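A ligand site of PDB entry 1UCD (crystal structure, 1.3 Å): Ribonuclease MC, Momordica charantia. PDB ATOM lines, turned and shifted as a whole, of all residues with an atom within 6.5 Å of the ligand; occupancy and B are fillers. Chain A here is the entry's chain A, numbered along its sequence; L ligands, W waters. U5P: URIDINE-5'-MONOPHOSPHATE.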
ATOM      1  N   GLN A   9       2.982 -31.270 -25.068  1.00  0.00           N
ATOM      2  CA  GLN A   9       2.036 -30.438 -25.788  1.00  0.00           C
ATOM      3  C   GLN A   9       2.489 -30.275 -27.229  1.00  0.00           C
ATOM      4  O   GLN A   9       3.675 -30.352 -27.543  1.00  0.00           O
ATOM      5  CB  GLN A   9       1.934 -29.072 -25.106  1.00  0.00           C
ATOM      6  CG  GLN A   9       3.239 -28.302 -25.059  1.00  0.00           C
ATOM      7  CD  GLN A   9       3.121 -26.991 -24.278  1.00  0.00           C
ATOM      8  OE1 GLN A   9       2.024 -26.498 -24.047  1.00  0.00           O
ATOM      9  NE2 GLN A   9       4.262 -26.432 -23.884  1.00  0.00           N
ATOM     10  N   VAL A  14      -1.335 -25.541 -29.263  1.00  0.00           N
ATOM     11  CA  VAL A  14      -1.426 -24.718 -28.074  1.00  0.00           C
ATOM     12  C   VAL A  14      -1.475 -23.247 -28.493  1.00  0.00           C
ATOM     13  O   VAL A  14      -2.273 -22.463 -27.986  1.00  0.00           O
ATOM     14  CB  VAL A  14      -0.219 -24.958 -27.139  1.00  0.00           C
ATOM     15  CG1 VAL A  14      -0.259 -23.992 -25.968  1.00  0.00           C
ATOM     16  CG2 VAL A  14      -0.225 -26.390 -26.643  1.00  0.00           C
ATOM     17  N   THR A  32       6.572 -31.036 -27.272  1.00  0.00           N
ATOM     18  CA  THR A  32       7.487 -30.562 -26.251  1.00  0.00           C
ATOM     19  C   THR A  32       6.865 -30.823 -24.903  1.00  0.00           C
ATOM     20  O   THR A  32       5.683 -31.125 -24.794  1.00  0.00           O
ATOM     21  CB  THR A  32       7.775 -29.070 -26.425  1.00  0.00           C
ATOM     22  OG1 THR A  32       6.551 -28.340 -26.403  1.00  0.00           O
ATOM     23  CG2 THR A  32       8.510 -28.820 -27.744  1.00  0.00           C
ATOM     24  N   ILE A  33       7.669 -30.699 -23.860  1.00  0.00           N
ATOM     25  CA  ILE A  33       7.180 -30.944 -22.522  1.00  0.00           C
ATOM     26  C   ILE A  33       6.370 -29.800 -21.960  1.00  0.00           C
ATOM     27  O   ILE A  33       6.792 -28.651 -22.001  1.00  0.00           O
ATOM     28  CB  ILE A  33       8.357 -31.168 -21.563  1.00  0.00           C
ATOM     29  CG1 ILE A  33       9.206 -32.340 -22.033  1.00  0.00           C
ATOM     30  CG2 ILE A  33       7.829 -31.378 -20.146  1.00  0.00           C
ATOM     31  CD1 ILE A  33      10.540 -32.415 -21.356  1.00  0.00           C
ATOM     32  N   HIS A  34       5.180 -30.100 -21.460  1.00  0.00           N
ATOM     33  CA  HIS A  34       4.416 -29.070 -20.789  1.00  0.00           C
ATOM     34  C   HIS A  34       4.868 -29.224 -19.345  1.00  0.00           C
ATOM     35  O   HIS A  34       5.340 -28.285 -18.724  1.00  0.00           O
ATOM     36  CB  HIS A  34       2.913 -29.308 -20.890  1.00  0.00           C
ATOM     37  CG  HIS A  34       2.099 -28.347 -20.074  1.00  0.00           C
ATOM     38  ND1 HIS A  34       0.728 -28.261 -20.186  1.00  0.00           N
ATOM     39  CD2 HIS A  34       2.456 -27.442 -19.140  1.00  0.00           C
ATOM     40  CE1 HIS A  34       0.286 -27.336 -19.347  1.00  0.00           C
ATOM     41  NE2 HIS A  34       1.312 -26.830 -18.704  1.00  0.00           N
ATOM     42  N   GLY A  35       4.744 -30.445 -18.820  1.00  0.00           N
ATOM     43  CA  GLY A  35       5.181 -30.678 -17.462  1.00  0.00           C
ATOM     44  C   GLY A  35       5.077 -32.123 -17.058  1.00  0.00           C
ATOM     45  O   GLY A  35       4.575 -32.964 -17.792  1.00  0.00           O
ATOM     46  N   TRP A  37       3.550 -34.057 -14.031  1.00  0.00           N
ATOM     47  CA  TRP A  37       2.625 -33.820 -12.943  1.00  0.00           C
ATOM     48  C   TRP A  37       2.397 -34.978 -12.004  1.00  0.00           C
ATOM     49  O   TRP A  37       1.773 -35.973 -12.374  1.00  0.00           O
ATOM     50  CB  TRP A  37       1.275 -33.389 -13.502  1.00  0.00           C
ATOM     51  CG  TRP A  37       1.344 -32.245 -14.454  1.00  0.00           C
ATOM     52  CD1 TRP A  37       2.372 -31.355 -14.612  1.00  0.00           C
ATOM     53  CD2 TRP A  37       0.319 -31.850 -15.368  1.00  0.00           C
ATOM     54  NE1 TRP A  37       2.035 -30.415 -15.566  1.00  0.00           N
ATOM     55  CE2 TRP A  37       0.777 -30.703 -16.046  1.00  0.00           C
ATOM     56  CE3 TRP A  37      -0.953 -32.360 -15.680  1.00  0.00           C
ATOM     57  CZ2 TRP A  37       0.021 -30.043 -17.021  1.00  0.00           C
ATOM     58  CZ3 TRP A  37      -1.711 -31.699 -16.642  1.00  0.00           C
ATOM     59  CH2 TRP A  37      -1.221 -30.561 -17.301  1.00  0.00           C
ATOM     60  N   PRO A  70      10.621 -26.006 -24.150  1.00  0.00           N
ATOM     61  CA  PRO A  70      10.565 -24.557 -24.348  1.00  0.00           C
ATOM     62  C   PRO A  70       9.222 -24.008 -23.903  1.00  0.00           C
ATOM     63  O   PRO A  70       8.227 -24.741 -23.822  1.00  0.00           O
ATOM     64  CB  PRO A  70      10.756 -24.419 -25.853  1.00  0.00           C
ATOM     65  CG  PRO A  70      10.038 -25.624 -26.373  1.00  0.00           C
ATOM     66  CD  PRO A  70      10.533 -26.714 -25.438  1.00  0.00           C
ATOM     67  N   ASN A  71       9.195 -22.724 -23.594  1.00  0.00           N
ATOM     68  CA  ASN A  71       7.955 -22.065 -23.251  1.00  0.00           C
ATOM     69  C   ASN A  71       7.434 -21.760 -24.650  1.00  0.00           C
ATOM     70  O   ASN A  71       8.043 -20.967 -25.378  1.00  0.00           O
ATOM     71  CB  ASN A  71       8.223 -20.786 -22.487  1.00  0.00           C
ATOM     72  CG  ASN A  71       6.950 -20.099 -22.071  1.00  0.00           C
ATOM     73  OD1 ASN A  71       5.903 -20.292 -22.674  1.00  0.00           O
ATOM     74  ND2 ASN A  71       7.044 -19.271 -21.028  1.00  0.00           N
ATOM     75  N   VAL A  72       6.323 -22.369 -25.052  1.00  0.00           N
ATOM     76  CA  VAL A  72       5.809 -22.141 -26.392  1.00  0.00           C
ATOM     77  C   VAL A  72       4.914 -20.925 -26.529  1.00  0.00           C
ATOM     78  O   VAL A  72       4.573 -20.530 -27.641  1.00  0.00           O
ATOM     79  CB  VAL A  72       5.038 -23.375 -26.919  1.00  0.00           C
ATOM     80  CG1 VAL A  72       5.899 -24.617 -26.757  1.00  0.00           C
ATOM     81  CG2 VAL A  72       3.714 -23.534 -26.197  1.00  0.00           C
ATOM     82  N   LEU A  73       4.529 -20.321 -25.403  1.00  0.00           N
ATOM     83  CA  LEU A  73       3.656 -19.163 -25.422  1.00  0.00           C
ATOM     84  C   LEU A  73       4.432 -17.851 -25.503  1.00  0.00           C
ATOM     85  O   LEU A  73       3.952 -16.875 -26.070  1.00  0.00           O
ATOM     86  CB  LEU A  73       2.772 -19.149 -24.180  1.00  0.00           C
ATOM     87  CG  LEU A  73       1.816 -20.343 -24.105  1.00  0.00           C
ATOM     88  CD1 LEU A  73       0.987 -20.243 -22.843  1.00  0.00           C
ATOM     89  CD2 LEU A  73       0.912 -20.354 -25.335  1.00  0.00           C
ATOM     90  N   ARG A  74       5.633 -17.849 -24.931  1.00  0.00           N
ATOM     91  CA  ARG A  74       6.470 -16.664 -24.944  1.00  0.00           C
ATOM     92  C   ARG A  74       7.914 -17.094 -24.750  1.00  0.00           C
ATOM     93  O   ARG A  74       8.186 -18.165 -24.202  1.00  0.00           O
ATOM     94  CB  ARG A  74       6.029 -15.683 -23.849  1.00  0.00           C
ATOM     95  CG  ARG A  74       6.141 -16.221 -22.443  1.00  0.00           C
ATOM     96  CD  ARG A  74       5.431 -15.297 -21.456  1.00  0.00           C
ATOM     97  NE  ARG A  74       3.979 -15.337 -21.640  1.00  0.00           N
ATOM     98  CZ  ARG A  74       3.209 -16.354 -21.286  1.00  0.00           C
ATOM     99  NH1 ARG A  74       1.896 -16.307 -21.489  1.00  0.00           N
ATOM    100  NH2 ARG A  74       3.743 -17.424 -20.717  1.00  0.00           N
ATOM    101  N   ASN A  76      10.357 -17.231 -22.805  1.00  0.00           N
ATOM    102  CA  ASN A  76      10.857 -17.215 -21.438  1.00  0.00           C
ATOM    103  C   ASN A  76      10.745 -18.626 -20.878  1.00  0.00           C
ATOM    104  O   ASN A  76       9.787 -18.963 -20.173  1.00  0.00           O
ATOM    105  CB  ASN A  76      10.037 -16.253 -20.580  1.00  0.00           C
ATOM    106  CG  ASN A  76      10.707 -15.951 -19.253  1.00  0.00           C
ATOM    107  OD1 ASN A  76      11.383 -16.817 -18.676  1.00  0.00           O
ATOM    108  ND2 ASN A  76      10.529 -14.732 -18.763  1.00  0.00           N
ATOM    109  N   GLN A  79      10.822 -19.078 -16.766  1.00  0.00           N
ATOM    110  CA  GLN A  79       9.581 -18.773 -16.079  1.00  0.00           C
ATOM    111  C   GLN A  79       8.659 -19.990 -16.113  1.00  0.00           C
ATOM    112  O   GLN A  79       7.979 -20.287 -15.136  1.00  0.00           O
ATOM    113  CB  GLN A  79       8.896 -17.574 -16.751  1.00  0.00           C
ATOM    114  CG  GLN A  79       7.641 -17.102 -16.049  1.00  0.00           C
ATOM    115  CD  GLN A  79       7.106 -15.812 -16.638  1.00  0.00           C
ATOM    116  OE1 GLN A  79       6.755 -15.750 -17.815  1.00  0.00           O
ATOM    117  NE2 GLN A  79       7.033 -14.774 -15.815  1.00  0.00           N
ATOM    118  N   PHE A  80       8.647 -20.669 -17.249  1.00  0.00           N
ATOM    119  CA  PHE A  80       7.815 -21.849 -17.428  1.00  0.00           C
ATOM    120  C   PHE A  80       8.334 -23.004 -16.573  1.00  0.00           C
ATOM    121  O   PHE A  80       7.559 -23.673 -15.893  1.00  0.00           O
ATOM    122  CB  PHE A  80       7.796 -22.211 -18.914  1.00  0.00           C
ATOM    123  CG  PHE A  80       6.841 -23.315 -19.270  1.00  0.00           C
ATOM    124  CD1 PHE A  80       5.630 -23.477 -18.589  1.00  0.00           C
ATOM    125  CD2 PHE A  80       7.132 -24.156 -20.331  1.00  0.00           C
ATOM    126  CE1 PHE A  80       4.731 -24.473 -18.975  1.00  0.00           C
ATOM    127  CE2 PHE A  80       6.245 -25.151 -20.722  1.00  0.00           C
ATOM    128  CZ  PHE A  80       5.048 -25.313 -20.047  1.00  0.00           C
ATOM    129  N   HIS A  83       7.568 -22.277 -12.983  1.00  0.00           N
ATOM    130  CA  HIS A  83       6.160 -22.477 -12.714  1.00  0.00           C
ATOM    131  C   HIS A  83       5.835 -23.967 -12.574  1.00  0.00           C
ATOM    132  O   HIS A  83       5.146 -24.371 -11.639  1.00  0.00           O
ATOM    133  CB  HIS A  83       5.309 -21.900 -13.844  1.00  0.00           C
ATOM    134  CG  HIS A  83       3.865 -22.253 -13.727  1.00  0.00           C
ATOM    135  ND1 HIS A  83       3.057 -21.755 -12.736  1.00  0.00           N
ATOM    136  CD2 HIS A  83       3.098 -23.127 -14.440  1.00  0.00           C
ATOM    137  CE1 HIS A  83       1.857 -22.303 -12.823  1.00  0.00           C
ATOM    138  NE2 HIS A  83       1.862 -23.139 -13.853  1.00  0.00           N
ATOM    139  N   GLU A  84       6.328 -24.769 -13.509  1.00  0.00           N
ATOM    140  CA  GLU A  84       6.064 -26.194 -13.469  1.00  0.00           C
ATOM    141  C   GLU A  84       6.702 -26.855 -12.260  1.00  0.00           C
ATOM    142  O   GLU A  84       6.136 -27.771 -11.674  1.00  0.00           O
ATOM    143  CB  GLU A  84       6.540 -26.848 -14.774  1.00  0.00           C
ATOM    144  CG  GLU A  84       5.672 -26.472 -15.980  1.00  0.00           C
ATOM    145  CD  GLU A  84       4.220 -26.870 -15.798  1.00  0.00           C
ATOM    146  OE1 GLU A  84       3.965 -28.052 -15.470  1.00  0.00           O
ATOM    147  OE2 GLU A  84       3.328 -26.021 -15.990  1.00  0.00           O
ATOM    148  N   LYS A  87       4.545 -25.557  -9.116  1.00  0.00           N
ATOM    149  CA  LYS A  87       3.201 -26.091  -9.088  1.00  0.00           C
ATOM    150  C   LYS A  87       3.117 -27.611  -9.093  1.00  0.00           C
ATOM    151  O   LYS A  87       2.201 -28.181  -8.513  1.00  0.00           O
ATOM    152  CB  LYS A  87       2.405 -25.540 -10.274  1.00  0.00           C
ATOM    153  CG  LYS A  87       0.983 -26.048 -10.336  1.00  0.00           C
ATOM    154  CD  LYS A  87       0.188 -25.290 -11.369  1.00  0.00           C
ATOM    155  CE  LYS A  87      -1.219 -25.822 -11.493  1.00  0.00           C
ATOM    156  NZ  LYS A  87      -2.016 -25.009 -12.449  1.00  0.00           N
ATOM    157  N   HIS A  88       4.071 -28.265  -9.739  1.00  0.00           N
ATOM    158  CA  HIS A  88       4.035 -29.721  -9.839  1.00  0.00           C
ATOM    159  C   HIS A  88       5.230 -30.467  -9.265  1.00  0.00           C
ATOM    160  O   HIS A  88       5.063 -31.411  -8.495  1.00  0.00           O
ATOM    161  CB  HIS A  88       3.889 -30.122 -11.306  1.00  0.00           C
ATOM    162  CG  HIS A  88       2.685 -29.536 -11.970  1.00  0.00           C
ATOM    163  ND1 HIS A  88       1.414 -30.023 -11.791  1.00  0.00           N
ATOM    164  CD2 HIS A  88       2.571 -28.498 -12.845  1.00  0.00           C
ATOM    165  CE1 HIS A  88       0.565 -29.333 -12.523  1.00  0.00           C
ATOM    166  NE2 HIS A  88       1.242 -28.399 -13.173  1.00  0.00           N
ATOM    167  N   ARG A 150      -5.466 -34.984 -24.441  1.00  0.00           N
ATOM    168  CA  ARG A 150      -6.087 -33.769 -23.970  1.00  0.00           C
ATOM    169  C   ARG A 150      -6.335 -32.816 -25.111  1.00  0.00           C
ATOM    170  O   ARG A 150      -5.463 -32.561 -25.947  1.00  0.00           O
ATOM    171  CB  ARG A 150      -5.210 -33.133 -22.900  1.00  0.00           C
ATOM    172  CG  ARG A 150      -5.114 -34.003 -21.646  1.00  0.00           C
ATOM    173  CD  ARG A 150      -3.964 -33.599 -20.755  1.00  0.00           C
ATOM    174  NE  ARG A 150      -4.140 -32.272 -20.168  1.00  0.00           N
ATOM    175  CZ  ARG A 150      -4.986 -31.991 -19.177  1.00  0.00           C
ATOM    176  NH1 ARG A 150      -5.755 -32.939 -18.660  1.00  0.00           N
ATOM    177  NH2 ARG A 150      -5.043 -30.756 -18.706  1.00  0.00           N
ATOM    178  N   GLN A 164      -2.480 -31.889 -26.067  1.00  0.00           N
ATOM    179  CA  GLN A 164      -1.507 -32.594 -25.261  1.00  0.00           C
ATOM    180  C   GLN A 164      -1.693 -34.089 -25.265  1.00  0.00           C
ATOM    181  O   GLN A 164      -2.809 -34.598 -25.442  1.00  0.00           O
ATOM    182  CB  GLN A 164      -1.553 -32.106 -23.815  1.00  0.00           C
ATOM    183  CG  GLN A 164      -1.350 -30.617 -23.693  1.00  0.00           C
ATOM    184  CD  GLN A 164      -1.457 -30.147 -22.269  1.00  0.00           C
ATOM    185  OE1 GLN A 164      -2.213 -30.701 -21.468  1.00  0.00           O
ATOM    186  NE2 GLN A 164      -0.710 -29.103 -21.948  1.00  0.00           N
HETATM  187  N1  U5P L   1       2.215 -22.308 -20.127  1.00  0.00           N
HETATM  188  C2  U5P L   1       3.369 -21.600 -20.478  1.00  0.00           C
HETATM  189  N3  U5P L   1       4.056 -22.100 -21.557  1.00  0.00           N
HETATM  190  C4  U5P L   1       3.712 -23.229 -22.314  1.00  0.00           C
HETATM  191  C5  U5P L   1       2.516 -23.898 -21.891  1.00  0.00           C
HETATM  192  C6  U5P L   1       1.833 -23.445 -20.846  1.00  0.00           C
HETATM  193  O2  U5P L   1       3.715 -20.609 -19.854  1.00  0.00           O
HETATM  194  O4  U5P L   1       4.435 -23.530 -23.236  1.00  0.00           O
HETATM  195  C1' U5P L   1       1.462 -21.805 -18.965  1.00  0.00           C
HETATM  196  C2' U5P L   1       0.018 -21.387 -19.180  1.00  0.00           C
HETATM  197  O2' U5P L   1      -0.110 -20.079 -19.763  1.00  0.00           O
HETATM  198  C3' U5P L   1      -0.630 -21.545 -17.801  1.00  0.00           C
HETATM  199  C4' U5P L   1       0.121 -22.755 -17.270  1.00  0.00           C
HETATM  200  O3' U5P L   1      -0.494 -20.334 -16.997  1.00  0.00           O
HETATM  201  O4' U5P L   1       1.459 -22.677 -17.860  1.00  0.00           O
HETATM  202  C5' U5P L   1      -0.406 -24.146 -17.603  1.00  0.00           C
HETATM  203  O5' U5P L   1       0.313 -25.184 -16.930  1.00  0.00           O
HETATM  204  P   U5P L   1      -0.163 -25.779 -15.511  1.00  0.00           P
HETATM  205  O1P U5P L   1      -1.542 -26.401 -15.450  1.00  0.00           O
HETATM  206  O2P U5P L   1      -0.174 -24.705 -14.474  1.00  0.00           O
HETATM  207  O3P U5P L   1       1.092 -26.795 -15.173  1.00  0.00           O
HETATM  208  O   HOH W   1      -2.655 -28.830 -14.354  1.00  0.00           O
HETATM  209  O   HOH W   2      -2.452 -18.603 -17.691  1.00  0.00           O
HETATM  210  O   HOH W   3       5.234 -19.931 -17.684  1.00  0.00           O
HETATM  211  O   HOH W   4      -2.532 -26.815 -18.189  1.00  0.00           O
HETATM  212  O   HOH W   5       1.470 -17.947 -19.275  1.00  0.00           O
HETATM  213  O   HOH W   6      -2.288 -20.261 -21.400  1.00  0.00           O
HETATM  214  O   HOH W   7       1.644 -20.189 -15.186  1.00  0.00           O
HETATM  215  O   HOH W   8      -3.653 -24.709 -15.237  1.00  0.00           O
HETATM  216  O   HOH W   9      -1.035 -24.730 -21.281  1.00  0.00           O
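The side-chain carboxylate (OE2) of Glu 84 sits close to an oxygen (O3P) of the ligand, at 2.5 Å.
O3P of the ligand is in hydrogen-bond range of NE2 of His 88.
An oxygen (O5') of the ligand sits at hydrogen-bond distance from a ring nitrogen (NE2) of His 34 (2.6 Å).
An oxygen (O2P) of the ligand sits at hydrogen-bond distance from a ring nitrogen (NE2) of His 83 (2.6 Å).
An oxygen (O2P) of the ligand is in salt-bridge range of the side-chain amino group of Lys 87.
OD1 of Asn 71 is in hydrogen-bond range of N3 of the ligand.
N of Val 72 sits at hydrogen-bond distance from O4 of the ligand (2.9 Å).
NE2 of Gln 9 is in hydrogen-bond range of O4 of the ligand.
The guanidinium group (NH2) of Arg 74 is in hydrogen-bond range of an oxygen (O2) of the ligand (3.3 Å).
NE2 of His 34 sits at hydrogen-bond distance from OE2 of Glu 84, 3.5 Å away.
The indole nitrogen (NE1) of Trp 37 lies within hydrogen-bond range of the side-chain carboxylate (OE1) of Glu 84.
NE2 of His 88 sits at hydrogen-bond distance from NE1 of Trp 37, 3.2 Å away.
The side-chain amide nitrogen of Gln 164 lies within hydrogen-bond range of a ring nitrogen (ND1) of His 34 (2.4 Å).
The backbone NH of Leu 73 is in hydrogen-bond range of the side-chain amide oxygen of Asn 71, at 3.1 Å.
The side-chain amide oxygen (OD1) of Asn 71 is in hydrogen-bond range of the backbone NH (N) of Arg 74, 3.3 Å away.
The backbone carbonyl oxygen of Asn 76 lies within hydrogen-bond range of the side-chain amide nitrogen of Asn 71 (2.9 Å).
N of Gln 9 is in hydrogen-bond range of O of Thr 32 (2.7 Å).
Residues that only touch the ligand: Trp 37, Leu 73 and Phe 80.
Within 4 Å of the ligand: Gln 9, His 34, Trp 37, Asn 71, Val 72, Leu 73, Arg 74, Phe 80, His 83, Glu 84, Lys 87 and His 88.
The nearest printed residue that does not touch the ligand is Pro 70 (4.02 Å).
Water W5 bridges O2' of the ligand (2.7 Å) and NH2 of Arg 74 (2.7 Å).
Water W8 bridges O1P of the ligand (2.7 Å) and NZ of Lys 87 (3.2 Å).
Water W7 bridges O3' of the ligand (2.8 Å) and ND1 of His 83 (3.2 Å).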
